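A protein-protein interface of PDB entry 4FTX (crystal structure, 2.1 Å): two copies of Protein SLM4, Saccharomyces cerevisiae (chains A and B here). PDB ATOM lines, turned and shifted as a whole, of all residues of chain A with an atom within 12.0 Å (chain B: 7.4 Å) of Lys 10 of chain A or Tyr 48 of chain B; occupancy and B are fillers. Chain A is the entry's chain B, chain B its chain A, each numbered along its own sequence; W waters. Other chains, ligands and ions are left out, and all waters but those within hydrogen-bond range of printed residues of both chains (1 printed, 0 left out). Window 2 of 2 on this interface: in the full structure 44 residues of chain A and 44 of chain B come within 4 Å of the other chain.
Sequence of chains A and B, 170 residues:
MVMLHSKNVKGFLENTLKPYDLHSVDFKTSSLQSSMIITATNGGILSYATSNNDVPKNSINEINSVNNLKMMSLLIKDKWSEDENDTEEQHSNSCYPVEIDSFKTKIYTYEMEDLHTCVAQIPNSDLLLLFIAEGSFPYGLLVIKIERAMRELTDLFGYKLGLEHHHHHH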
ATOM      1  N   HIS A   5      12.531  17.006   1.448  1.00  0.00           N
ATOM      2  CA  HIS A   5      11.820  15.813   0.952  1.00  0.00           C
ATOM      3  C   HIS A   5      10.348  15.872   1.321  1.00  0.00           C
ATOM      4  O   HIS A   5       9.948  16.666   2.174  1.00  0.00           O
ATOM      5  CB  HIS A   5      12.464  14.544   1.516  1.00  0.00           C
ATOM      6  CG  HIS A   5      12.431  13.372   0.571  1.00  0.00           C
ATOM      7  ND1 HIS A   5      13.116  13.359  -0.608  1.00  0.00           N
ATOM      8  CD2 HIS A   5      11.791  12.158   0.656  1.00  0.00           C
ATOM      9  CE1 HIS A   5      12.906  12.198  -1.231  1.00  0.00           C
ATOM     10  NE2 HIS A   5      12.101  11.457  -0.470  1.00  0.00           N
ATOM     11  N   SER A   6       9.539  15.042   0.666  1.00  0.00           N
ATOM     12  CA  SER A   6       8.114  14.918   0.980  1.00  0.00           C
ATOM     13  C   SER A   6       7.628  13.499   0.709  1.00  0.00           C
ATOM     14  O   SER A   6       8.385  12.659   0.219  1.00  0.00           O
ATOM     15  CB  SER A   6       7.288  15.910   0.166  1.00  0.00           C
ATOM     16  OG  SER A   6       7.324  15.580  -1.209  1.00  0.00           O
ATOM     17  N   LYS A   7       6.362  13.239   1.025  1.00  0.00           N
ATOM     18  CA  LYS A   7       5.780  11.907   0.863  1.00  0.00           C
ATOM     19  C   LYS A   7       5.731  11.472  -0.599  1.00  0.00           C
ATOM     20  O   LYS A   7       6.328  10.462  -0.980  1.00  0.00           O
ATOM     21  CB  LYS A   7       4.371  11.854   1.466  1.00  0.00           C
ATOM     22  CG  LYS A   7       4.275  11.121   2.794  1.00  0.00           C
ATOM     23  CD  LYS A   7       4.871  11.917   3.944  1.00  0.00           C
ATOM     24  CE  LYS A   7       4.657  11.187   5.264  1.00  0.00           C
ATOM     25  NZ  LYS A   7       5.169  11.958   6.429  1.00  0.00           N
ATOM     26  N   ASN A   8       5.027  12.250  -1.412  1.00  0.00           N
ATOM     27  CA  ASN A   8       4.727  11.850  -2.777  1.00  0.00           C
ATOM     28  C   ASN A   8       4.981  12.955  -3.791  1.00  0.00           C
ATOM     29  O   ASN A   8       5.531  14.004  -3.454  1.00  0.00           O
ATOM     30  CB  ASN A   8       3.283  11.331  -2.863  1.00  0.00           C
ATOM     31  CG  ASN A   8       2.257  12.294  -2.264  1.00  0.00           C
ATOM     32  OD1 ASN A   8       2.517  13.486  -2.079  1.00  0.00           O
ATOM     33  ND2 ASN A   8       1.071  11.770  -1.968  1.00  0.00           N
ATOM     34  N   VAL A   9       4.576  12.718  -5.034  1.00  0.00           N
ATOM     35  CA  VAL A   9       4.826  13.671  -6.110  1.00  0.00           C
ATOM     36  C   VAL A   9       4.005  14.953  -5.917  1.00  0.00           C
ATOM     37  O   VAL A   9       4.533  16.048  -6.070  1.00  0.00           O
ATOM     38  CB  VAL A   9       4.553  13.060  -7.505  1.00  0.00           C
ATOM     39  CG1 VAL A   9       4.848  14.072  -8.587  1.00  0.00           C
ATOM     40  CG2 VAL A   9       5.394  11.814  -7.724  1.00  0.00           C
ATOM     41  N   LYS A  10       2.724  14.807  -5.573  1.00  0.00           N
ATOM     42  CA  LYS A  10       1.862  15.953  -5.272  1.00  0.00           C
ATOM     43  C   LYS A  10       2.485  16.880  -4.223  1.00  0.00           C
ATOM     44  O   LYS A  10       2.572  18.084  -4.432  1.00  0.00           O
ATOM     45  CB  LYS A  10       0.484  15.494  -4.785  1.00  0.00           C
ATOM     46  CG  LYS A  10      -0.545  16.617  -4.708  1.00  0.00           C
ATOM     47  CD  LYS A  10      -1.238  16.844  -6.047  1.00  0.00           C
ATOM     48  CE  LYS A  10      -2.488  17.713  -5.910  1.00  0.00           C
ATOM     49  NZ  LYS A  10      -2.151  19.155  -5.694  1.00  0.00           N
ATOM     50  N   GLY A  11       2.921  16.301  -3.107  1.00  0.00           N
ATOM     51  CA  GLY A  11       3.540  17.051  -2.026  1.00  0.00           C
ATOM     52  C   GLY A  11       4.843  17.715  -2.453  1.00  0.00           C
ATOM     53  O   GLY A  11       5.123  18.845  -2.062  1.00  0.00           O
ATOM     54  N   PHE A  12       5.628  17.021  -3.273  1.00  0.00           N
ATOM     55  CA  PHE A  12       6.836  17.602  -3.870  1.00  0.00           C
ATOM     56  C   PHE A  12       6.505  18.839  -4.710  1.00  0.00           C
ATOM     57  O   PHE A  12       7.198  19.858  -4.636  1.00  0.00           O
ATOM     58  CB  PHE A  12       7.581  16.551  -4.714  1.00  0.00           C
ATOM     59  CG  PHE A  12       8.576  17.141  -5.679  1.00  0.00           C
ATOM     60  CD1 PHE A  12       9.878  17.409  -5.277  1.00  0.00           C
ATOM     61  CD2 PHE A  12       8.208  17.435  -6.988  1.00  0.00           C
ATOM     62  CE1 PHE A  12      10.793  17.971  -6.156  1.00  0.00           C
ATOM     63  CE2 PHE A  12       9.121  17.988  -7.873  1.00  0.00           C
ATOM     64  CZ  PHE A  12      10.418  18.257  -7.454  1.00  0.00           C
ATOM     65  N   LEU A  13       5.449  18.743  -5.519  1.00  0.00           N
ATOM     66  CA  LEU A  13       5.058  19.869  -6.371  1.00  0.00           C
ATOM     67  C   LEU A  13       4.531  21.043  -5.539  1.00  0.00           C
ATOM     68  O   LEU A  13       4.824  22.202  -5.835  1.00  0.00           O
ATOM     69  CB  LEU A  13       4.031  19.441  -7.427  1.00  0.00           C
ATOM     70  CG  LEU A  13       4.565  18.499  -8.503  1.00  0.00           C
ATOM     71  CD1 LEU A  13       3.487  18.143  -9.503  1.00  0.00           C
ATOM     72  CD2 LEU A  13       5.759  19.116  -9.207  1.00  0.00           C
ATOM     73  N   GLU A  14       3.758  20.736  -4.506  1.00  0.00           N
ATOM     74  CA  GLU A  14       3.291  21.750  -3.558  1.00  0.00           C
ATOM     75  C   GLU A  14       4.474  22.428  -2.874  1.00  0.00           C
ATOM     76  O   GLU A  14       4.435  23.624  -2.605  1.00  0.00           O
ATOM     77  CB  GLU A  14       2.383  21.136  -2.492  1.00  0.00           C
ATOM     78  CG  GLU A  14       1.126  20.455  -3.027  1.00  0.00           C
ATOM     79  CD  GLU A  14      -0.049  21.399  -3.236  1.00  0.00           C
ATOM     80  OE1 GLU A  14       0.151  22.635  -3.269  1.00  0.00           O
ATOM     81  OE2 GLU A  14      -1.187  20.895  -3.363  1.00  0.00           O
ATOM     82  N   ASN A  15       5.525  21.665  -2.590  1.00  0.00           N
ATOM     83  CA  ASN A  15       6.700  22.254  -1.956  1.00  0.00           C
ATOM     84  C   ASN A  15       7.442  23.199  -2.886  1.00  0.00           C
ATOM     85  O   ASN A  15       7.941  24.227  -2.432  1.00  0.00           O
ATOM     86  CB  ASN A  15       7.639  21.194  -1.384  1.00  0.00           C
ATOM     87  CG  ASN A  15       7.166  20.663  -0.045  1.00  0.00           C
ATOM     88  OD1 ASN A  15       6.392  21.314   0.655  1.00  0.00           O
ATOM     89  ND2 ASN A  15       7.641  19.479   0.325  1.00  0.00           N
ATOM     90  N   THR A  16       7.489  22.872  -4.182  1.00  0.00           N
ATOM     91  CA  THR A  16       8.109  23.778  -5.151  1.00  0.00           C
ATOM     92  C   THR A  16       7.425  25.149  -5.220  1.00  0.00           C
ATOM     93  O   THR A  16       8.046  26.126  -5.638  1.00  0.00           O
ATOM     94  CB  THR A  16       8.212  23.193  -6.585  1.00  0.00           C
ATOM     95  OG1 THR A  16       6.899  22.976  -7.111  1.00  0.00           O
ATOM     96  CG2 THR A  16       9.010  21.886  -6.605  1.00  0.00           C
ATOM     97  N   LEU A  17       6.166  25.231  -4.796  1.00  0.00           N
ATOM     98  CA  LEU A  17       5.435  26.502  -4.817  1.00  0.00           C
ATOM     99  C   LEU A  17       5.872  27.484  -3.716  1.00  0.00           C
ATOM    100  O   LEU A  17       5.638  28.685  -3.836  1.00  0.00           O
ATOM    101  CB  LEU A  17       3.921  26.273  -4.704  1.00  0.00           C
ATOM    102  CG  LEU A  17       3.218  25.404  -5.751  1.00  0.00           C
ATOM    103  CD1 LEU A  17       1.722  25.430  -5.486  1.00  0.00           C
ATOM    104  CD2 LEU A  17       3.528  25.876  -7.164  1.00  0.00           C
ATOM    105  N   LYS A  18       6.457  26.974  -2.633  1.00  0.00           N
ATOM    106  CA  LYS A  18       6.906  27.823  -1.528  1.00  0.00           C
ATOM    107  C   LYS A  18       8.007  28.782  -1.997  1.00  0.00           C
ATOM    108  O   LYS A  18       8.718  28.480  -2.959  1.00  0.00           O
ATOM    109  CB  LYS A  18       7.413  26.964  -0.365  1.00  0.00           C
ATOM    110  CG  LYS A  18       6.334  26.159   0.344  1.00  0.00           C
ATOM    111  CD  LYS A  18       6.963  25.209   1.353  1.00  0.00           C
ATOM    112  CE  LYS A  18       5.913  24.496   2.195  1.00  0.00           C
ATOM    113  NZ  LYS A  18       4.990  23.677   1.366  1.00  0.00           N
ATOM    114  N   SER B  34       2.624  27.994 -10.596  1.00  0.00           N
ATOM    115  CA  SER B  34       2.219  26.597 -10.640  1.00  0.00           C
ATOM    116  C   SER B  34       3.376  25.687 -10.980  1.00  0.00           C
ATOM    117  O   SER B  34       4.420  26.130 -11.465  1.00  0.00           O
ATOM    118  CB  SER B  34       1.024  26.396 -11.582  1.00  0.00           C
ATOM    119  OG  SER B  34       1.386  26.579 -12.933  1.00  0.00           O
ATOM    120  N   SER B  35       3.198  24.409 -10.690  1.00  0.00           N
ATOM    121  CA  SER B  35       4.264  23.442 -10.875  1.00  0.00           C
ATOM    122  C   SER B  35       3.620  22.121 -11.276  1.00  0.00           C
ATOM    123  O   SER B  35       2.648  21.694 -10.658  1.00  0.00           O
ATOM    124  CB  SER B  35       5.016  23.265  -9.561  1.00  0.00           C
ATOM    125  OG  SER B  35       6.166  22.463  -9.741  1.00  0.00           O
ATOM    126  N   MET B  36       4.138  21.479 -12.311  1.00  0.00           N
ATOM    127  CA  MET B  36       3.557  20.209 -12.684  1.00  0.00           C
ATOM    128  C   MET B  36       4.486  19.214 -13.340  1.00  0.00           C
ATOM    129  O   MET B  36       5.569  19.551 -13.814  1.00  0.00           O
ATOM    130  CB  MET B  36       2.296  20.413 -13.517  1.00  0.00           C
ATOM    131  CG  MET B  36       2.474  21.029 -14.868  1.00  0.00           C
ATOM    132  SD  MET B  36       1.169  22.277 -15.081  1.00  0.00           S
ATOM    133  CE  MET B  36       2.140  23.713 -14.615  1.00  0.00           C
ATOM    134  N   ILE B  37       4.049  17.963 -13.316  1.00  0.00           N
ATOM    135  CA  ILE B  37       4.684  16.909 -14.087  1.00  0.00           C
ATOM    136  C   ILE B  37       3.704  16.502 -15.166  1.00  0.00           C
ATOM    137  O   ILE B  37       2.534  16.134 -14.883  1.00  0.00           O
ATOM    138  CB  ILE B  37       5.119  15.745 -13.202  1.00  0.00           C
ATOM    139  CG1 ILE B  37       6.245  16.237 -12.265  1.00  0.00           C
ATOM    140  CG2 ILE B  37       5.586  14.564 -14.050  1.00  0.00           C
ATOM    141  CD1 ILE B  37       6.810  15.193 -11.342  1.00  0.00           C
ATOM    142  N   ILE B  38       4.188  16.618 -16.401  1.00  0.00           N
ATOM    143  CA  ILE B  38       3.389  16.345 -17.593  1.00  0.00           C
ATOM    144  C   ILE B  38       4.074  15.313 -18.481  1.00  0.00           C
ATOM    145  O   ILE B  38       5.257  15.036 -18.309  1.00  0.00           O
ATOM    146  CB  ILE B  38       3.127  17.623 -18.399  1.00  0.00           C
ATOM    147  CG1 ILE B  38       4.418  18.145 -19.040  1.00  0.00           C
ATOM    148  CG2 ILE B  38       2.506  18.709 -17.516  1.00  0.00           C
ATOM    149  CD1 ILE B  38       4.210  19.418 -19.836  1.00  0.00           C
ATOM    150  N   ILE B  45      -1.211  16.418 -18.266  1.00  0.00           N
ATOM    151  CA  ILE B  45      -0.811  16.652 -16.888  1.00  0.00           C
ATOM    152  C   ILE B  45      -1.029  15.395 -16.077  1.00  0.00           C
ATOM    153  O   ILE B  45      -2.128  14.813 -16.088  1.00  0.00           O
ATOM    154  CB  ILE B  45      -1.612  17.793 -16.243  1.00  0.00           C
ATOM    155  CG1 ILE B  45      -1.282  19.117 -16.917  1.00  0.00           C
ATOM    156  CG2 ILE B  45      -1.341  17.859 -14.738  1.00  0.00           C
ATOM    157  CD1 ILE B  45      -2.177  20.254 -16.468  1.00  0.00           C
ATOM    158  N   LEU B  46       0.007  14.974 -15.360  1.00  0.00           N
ATOM    159  CA  LEU B  46      -0.102  13.787 -14.526  1.00  0.00           C
ATOM    160  C   LEU B  46      -0.131  14.140 -13.054  1.00  0.00           C
ATOM    161  O   LEU B  46      -0.691  13.406 -12.243  1.00  0.00           O
ATOM    162  CB  LEU B  46       1.037  12.812 -14.826  1.00  0.00           C
ATOM    163  CG  LEU B  46       0.924  12.066 -16.158  1.00  0.00           C
ATOM    164  CD1 LEU B  46       2.141  11.192 -16.345  1.00  0.00           C
ATOM    165  CD2 LEU B  46      -0.357  11.225 -16.238  1.00  0.00           C
ATOM    166  N   SER B  47       0.482  15.268 -12.710  1.00  0.00           N
ATOM    167  CA  SER B  47       0.404  15.794 -11.343  1.00  0.00           C
ATOM    168  C   SER B  47       0.635  17.298 -11.387  1.00  0.00           C
ATOM    169  O   SER B  47       1.401  17.776 -12.211  1.00  0.00           O
ATOM    170  CB  SER B  47       1.454  15.128 -10.444  1.00  0.00           C
ATOM    171  OG  SER B  47       1.264  15.476  -9.070  1.00  0.00           O
ATOM    172  N   TYR B  48      -0.020  18.048 -10.510  1.00  0.00           N
ATOM    173  CA  TYR B  48       0.175  19.496 -10.488  1.00  0.00           C
ATOM    174  C   TYR B  48      -0.099  20.082  -9.115  1.00  0.00           C
ATOM    175  O   TYR B  48      -0.775  19.474  -8.286  1.00  0.00           O
ATOM    176  CB  TYR B  48      -0.733  20.194 -11.516  1.00  0.00           C
ATOM    177  CG  TYR B  48      -2.170  20.409 -11.021  1.00  0.00           C
ATOM    178  CD1 TYR B  48      -3.124  19.390 -11.075  1.00  0.00           C
ATOM    179  CD2 TYR B  48      -2.567  21.640 -10.512  1.00  0.00           C
ATOM    180  CE1 TYR B  48      -4.439  19.611 -10.631  1.00  0.00           C
ATOM    181  CE2 TYR B  48      -3.857  21.868 -10.071  1.00  0.00           C
ATOM    182  CZ  TYR B  48      -4.787  20.856 -10.129  1.00  0.00           C
ATOM    183  OH  TYR B  48      -6.053  21.116  -9.682  1.00  0.00           O
ATOM    184  N   ALA B  49       0.420  21.288  -8.907  1.00  0.00           N
ATOM    185  CA  ALA B  49       0.074  22.140  -7.771  1.00  0.00           C
ATOM    186  C   ALA B  49       0.009  23.579  -8.266  1.00  0.00           C
ATOM    187  O   ALA B  49       0.793  23.964  -9.142  1.00  0.00           O
ATOM    188  CB  ALA B  49       1.137  22.016  -6.685  1.00  0.00           C
ATOM    189  N   THR B  50      -0.919  24.363  -7.714  1.00  0.00           N
ATOM    190  CA  THR B  50      -1.034  25.801  -8.010  1.00  0.00           C
ATOM    191  C   THR B  50      -1.255  26.564  -6.728  1.00  0.00           C
ATOM    192  O   THR B  50      -1.951  26.080  -5.839  1.00  0.00           O
ATOM    193  CB  THR B  50      -2.251  26.147  -8.885  1.00  0.00           C
ATOM    194  OG1 THR B  50      -3.417  25.520  -8.347  1.00  0.00           O
ATOM    195  CG2 THR B  50      -2.065  25.681 -10.284  1.00  0.00           C
ATOM    196  N   LYS B  57     -10.505  29.202  -3.022  1.00  0.00           N
ATOM    197  CA  LYS B  57     -10.506  27.801  -3.437  1.00  0.00           C
ATOM    198  C   LYS B  57     -11.934  27.271  -3.466  1.00  0.00           C
ATOM    199  O   LYS B  57     -12.421  26.708  -2.479  1.00  0.00           O
ATOM    200  CB  LYS B  57      -9.647  26.944  -2.502  1.00  0.00           C
ATOM    201  CG  LYS B  57      -8.176  27.333  -2.468  1.00  0.00           C
ATOM    202  CD  LYS B  57      -7.302  26.165  -2.033  1.00  0.00           C
ATOM    203  CE  LYS B  57      -7.148  25.143  -3.157  1.00  0.00           C
ATOM    204  NZ  LYS B  57      -6.185  24.062  -2.810  1.00  0.00           N
ATOM    205  N   GLU B  62     -11.634  26.231  -9.508  1.00  0.00           N
ATOM    206  CA  GLU B  62     -10.830  25.039  -9.631  1.00  0.00           C
ATOM    207  C   GLU B  62     -10.904  24.488 -11.055  1.00  0.00           C
ATOM    208  O   GLU B  62      -9.871  24.175 -11.657  1.00  0.00           O
ATOM    209  CB  GLU B  62     -11.218  23.970  -8.596  1.00  0.00           C
ATOM    210  CG  GLU B  62     -10.088  22.956  -8.395  1.00  0.00           C
ATOM    211  CD  GLU B  62     -10.512  21.664  -7.712  1.00  0.00           C
ATOM    212  OE1 GLU B  62     -11.213  21.744  -6.674  1.00  0.00           O
ATOM    213  OE2 GLU B  62     -10.113  20.573  -8.211  1.00  0.00           O
ATOM    214  N   ILE B  63     -12.117  24.379 -11.593  1.00  0.00           N
ATOM    215  CA  ILE B  63     -12.293  23.778 -12.918  1.00  0.00           C
ATOM    216  C   ILE B  63     -11.557  24.625 -13.963  1.00  0.00           C
ATOM    217  O   ILE B  63     -10.776  24.102 -14.771  1.00  0.00           O
ATOM    218  CB  ILE B  63     -13.777  23.593 -13.291  1.00  0.00           C
ATOM    219  CG1 ILE B  63     -14.482  22.649 -12.306  1.00  0.00           C
ATOM    220  CG2 ILE B  63     -13.899  23.046 -14.695  1.00  0.00           C
ATOM    221  CD1 ILE B  63     -13.787  21.304 -12.114  1.00  0.00           C
ATOM    222  N   SER B  65      -9.109  26.918 -13.622  1.00  0.00           N
ATOM    223  CA  SER B  65      -7.656  26.981 -13.549  1.00  0.00           C
ATOM    224  C   SER B  65      -7.046  25.669 -14.028  1.00  0.00           C
ATOM    225  O   SER B  65      -6.000  25.695 -14.660  1.00  0.00           O
ATOM    226  CB  SER B  65      -7.160  27.354 -12.148  1.00  0.00           C
ATOM    227  OG  SER B  65      -7.373  26.295 -11.242  1.00  0.00           O
ATOM    228  N   VAL B  66      -7.702  24.529 -13.785  1.00  0.00           N
ATOM    229  CA  VAL B  66      -7.121  23.272 -14.289  1.00  0.00           C
ATOM    230  C   VAL B  66      -7.145  23.256 -15.801  1.00  0.00           C
ATOM    231  O   VAL B  66      -6.173  22.862 -16.435  1.00  0.00           O
ATOM    232  CB  VAL B  66      -7.827  21.990 -13.773  1.00  0.00           C
ATOM    233  CG1 VAL B  66      -7.256  20.757 -14.480  1.00  0.00           C
ATOM    234  CG2 VAL B  66      -7.627  21.854 -12.286  1.00  0.00           C
ATOM    235  N   LEU B  69      -4.291  25.381 -17.023  1.00  0.00           N
ATOM    236  CA  LEU B  69      -3.021  24.664 -16.859  1.00  0.00           C
ATOM    237  C   LEU B  69      -2.827  23.617 -17.949  1.00  0.00           C
ATOM    238  O   LEU B  69      -1.726  23.467 -18.460  1.00  0.00           O
ATOM    239  CB  LEU B  69      -2.936  23.982 -15.498  1.00  0.00           C
ATOM    240  CG  LEU B  69      -2.807  24.836 -14.245  1.00  0.00           C
ATOM    241  CD1 LEU B  69      -2.743  23.892 -13.074  1.00  0.00           C
ATOM    242  CD2 LEU B  69      -1.574  25.746 -14.291  1.00  0.00           C
ATOM    243  N   SER B  73       0.262  23.632 -20.496  1.00  0.00           N
ATOM    244  CA  SER B  73       1.095  22.441 -20.527  1.00  0.00           C
ATOM    245  C   SER B  73       1.234  21.935 -21.945  1.00  0.00           C
ATOM    246  O   SER B  73       2.322  21.554 -22.358  1.00  0.00           O
ATOM    247  CB  SER B  73       0.491  21.350 -19.655  1.00  0.00           C
ATOM    248  OG  SER B  73       0.710  21.655 -18.298  1.00  0.00           O
HETATM  249  O   HOH W   1      -2.528  22.767  -5.610  1.00  0.00           O
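The side-chain hydroxyl of Thr 16 of chain A lies within hydrogen-bond range of the side-chain hydroxyl of Ser 35 of chain B (2.8 Å). The backbone carbonyl oxygen (O) of Tyr 48 of chain B is in hydrogen-bond range of the side-chain amino group (NZ) of Lys 10 of chain A, 3.0 Å away.
O of Leu 13 of chain A lies within hydrogen-bond range of OG1 of Thr 16 of chain A. NZ of Lys 10 of chain A is in salt-bridge range of OE2 of Glu 14 of chain A (3.1 Å). SD of Met 36 of chain B is in hydrogen-bond range of OG of Ser 73 of chain B, at 3.3 Å. The backbone NH of Leu 46 of chain B is in hydrogen-bond range of the backbone carbonyl oxygen of Ile 37 of chain B, at 2.8 Å. N of Ala 49 of chain B is in hydrogen-bond range of O of Ser 35 of chain B. O of Ser 47 of chain B lies within hydrogen-bond range of N of Ile 37 of chain B, 2.9 Å away.
Among the printed residues, pairs that only touch across the chains: Leu 13 of chain A with Ser 35 of chain B (3.4 Å), Leu 17 of chain A with Thr 50 of chain B (3.4 Å), Leu 13 of chain A with Ser 47 of chain B (3.4 Å), Val 9 of chain A with Ile 37 of chain B (3.6 Å), Glu 14 of chain A with Ala 49 of chain B (3.6 Å), Leu 13 of chain A with Tyr 48 of chain B (3.6 Å), Leu 17 of chain A with Ala 49 of chain B (3.7 Å), Leu 13 of chain A with Ala 49 of chain B (3.7 Å), Leu 17 of chain A with Ser 34 of chain B (3.8 Å), Leu 13 of chain A with Met 36 of chain B (3.8 Å), Leu 17 of chain A with Ser 35 of chain B (3.8 Å), Lys 10 of chain A with Ser 47 of chain B (3.8 Å), Leu 13 of chain A with Ile 37 of chain B (3.9 Å) and Val 9 of chain A with Ser 47 of chain B (3.9 Å).
Ser 6 of chain A touches none of the printed residues of chain B. Asn 8 of chain A touches none of the printed residues of chain B. Printed residues of chain B within 4 Å of Val 9 of chain A: Ile 37 and Ser 47. Printed residues of chain B within 4 Å of Leu 13 of chain A: Ser 35, Met 36, Ile 37, Ser 47, Tyr 48 and Ala 49. Printed residues of chain B within 4 Å of Glu 14 of chain A: Ala 49 (3.6 Å). Printed residues of chain B within 4 Å of Leu 17 of chain A: Ser 34 (3.8 Å), Ser 35 (3.8 Å), Ala 49 (3.7 Å) and Thr 50 (3.4 Å). Of the printed residues of chain A, Ser 34 of chain B touches Leu 17 (3.8 Å). Ser 35 of chain B touches just these residues of chain A: Leu 13 (3.4 Å), Thr 16 (2.8 Å) and Leu 17 (3.8 Å). Of the printed residues of chain A, Met 36 of chain B touches Leu 13 (3.8 Å). Of the printed residues of chain A, Tyr 48 of chain B touches Lys 10 and Leu 13. Of chain A, only Leu 13 (3.7 Å), Glu 14 (3.6 Å) and Leu 17 (3.7 Å) come within 4 Å of Ala 49 of chain B. Thr 50 of chain B touches just one residue of chain A: Leu 17 (3.4 Å). No residue of chain A comes within 4 Å of Glu 62 of chain B. No residue of chain A comes within 4 Å of Ser 65 of chain B. No residue of chain A comes within 4 Å of Val 66 of chain B. No residue of chain A comes within 4 Å of Leu 69 of chain B. The nearest residue of chain B that does not touch Lys 10 of chain A is Ala 49 of chain B (4.3 Å). The nearest residue of chain A that does not touch Tyr 48 of chain B is Glu 14 of chain A (5.1 Å).
Printed residues of chain A that touch a printed residue of chain B: Val 9, Lys 10, Leu 13, Glu 14, Thr 16 and Leu 17. Printed residues of chain B that touch a printed residue of chain A: Ser 34, Ser 35, Met 36, Ile 37, Ser 47, Tyr 48, Ala 49 and Thr 50. Hydrophobic or aromatic side chains of chain B that line the printed part of chain A: Ile 37 and Ala 49. Among the printed residues, no Asp or Glu carboxylate lies within 4 Å of a Lys or Arg side-chain nitrogen of the other chain.
No position is printed for both chains.
Water W1 lies within hydrogen-bond range of the backbone NH (N) of Thr 50 of chain B and the side-chain carboxylate (OE2) of Glu 14 of chain A.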
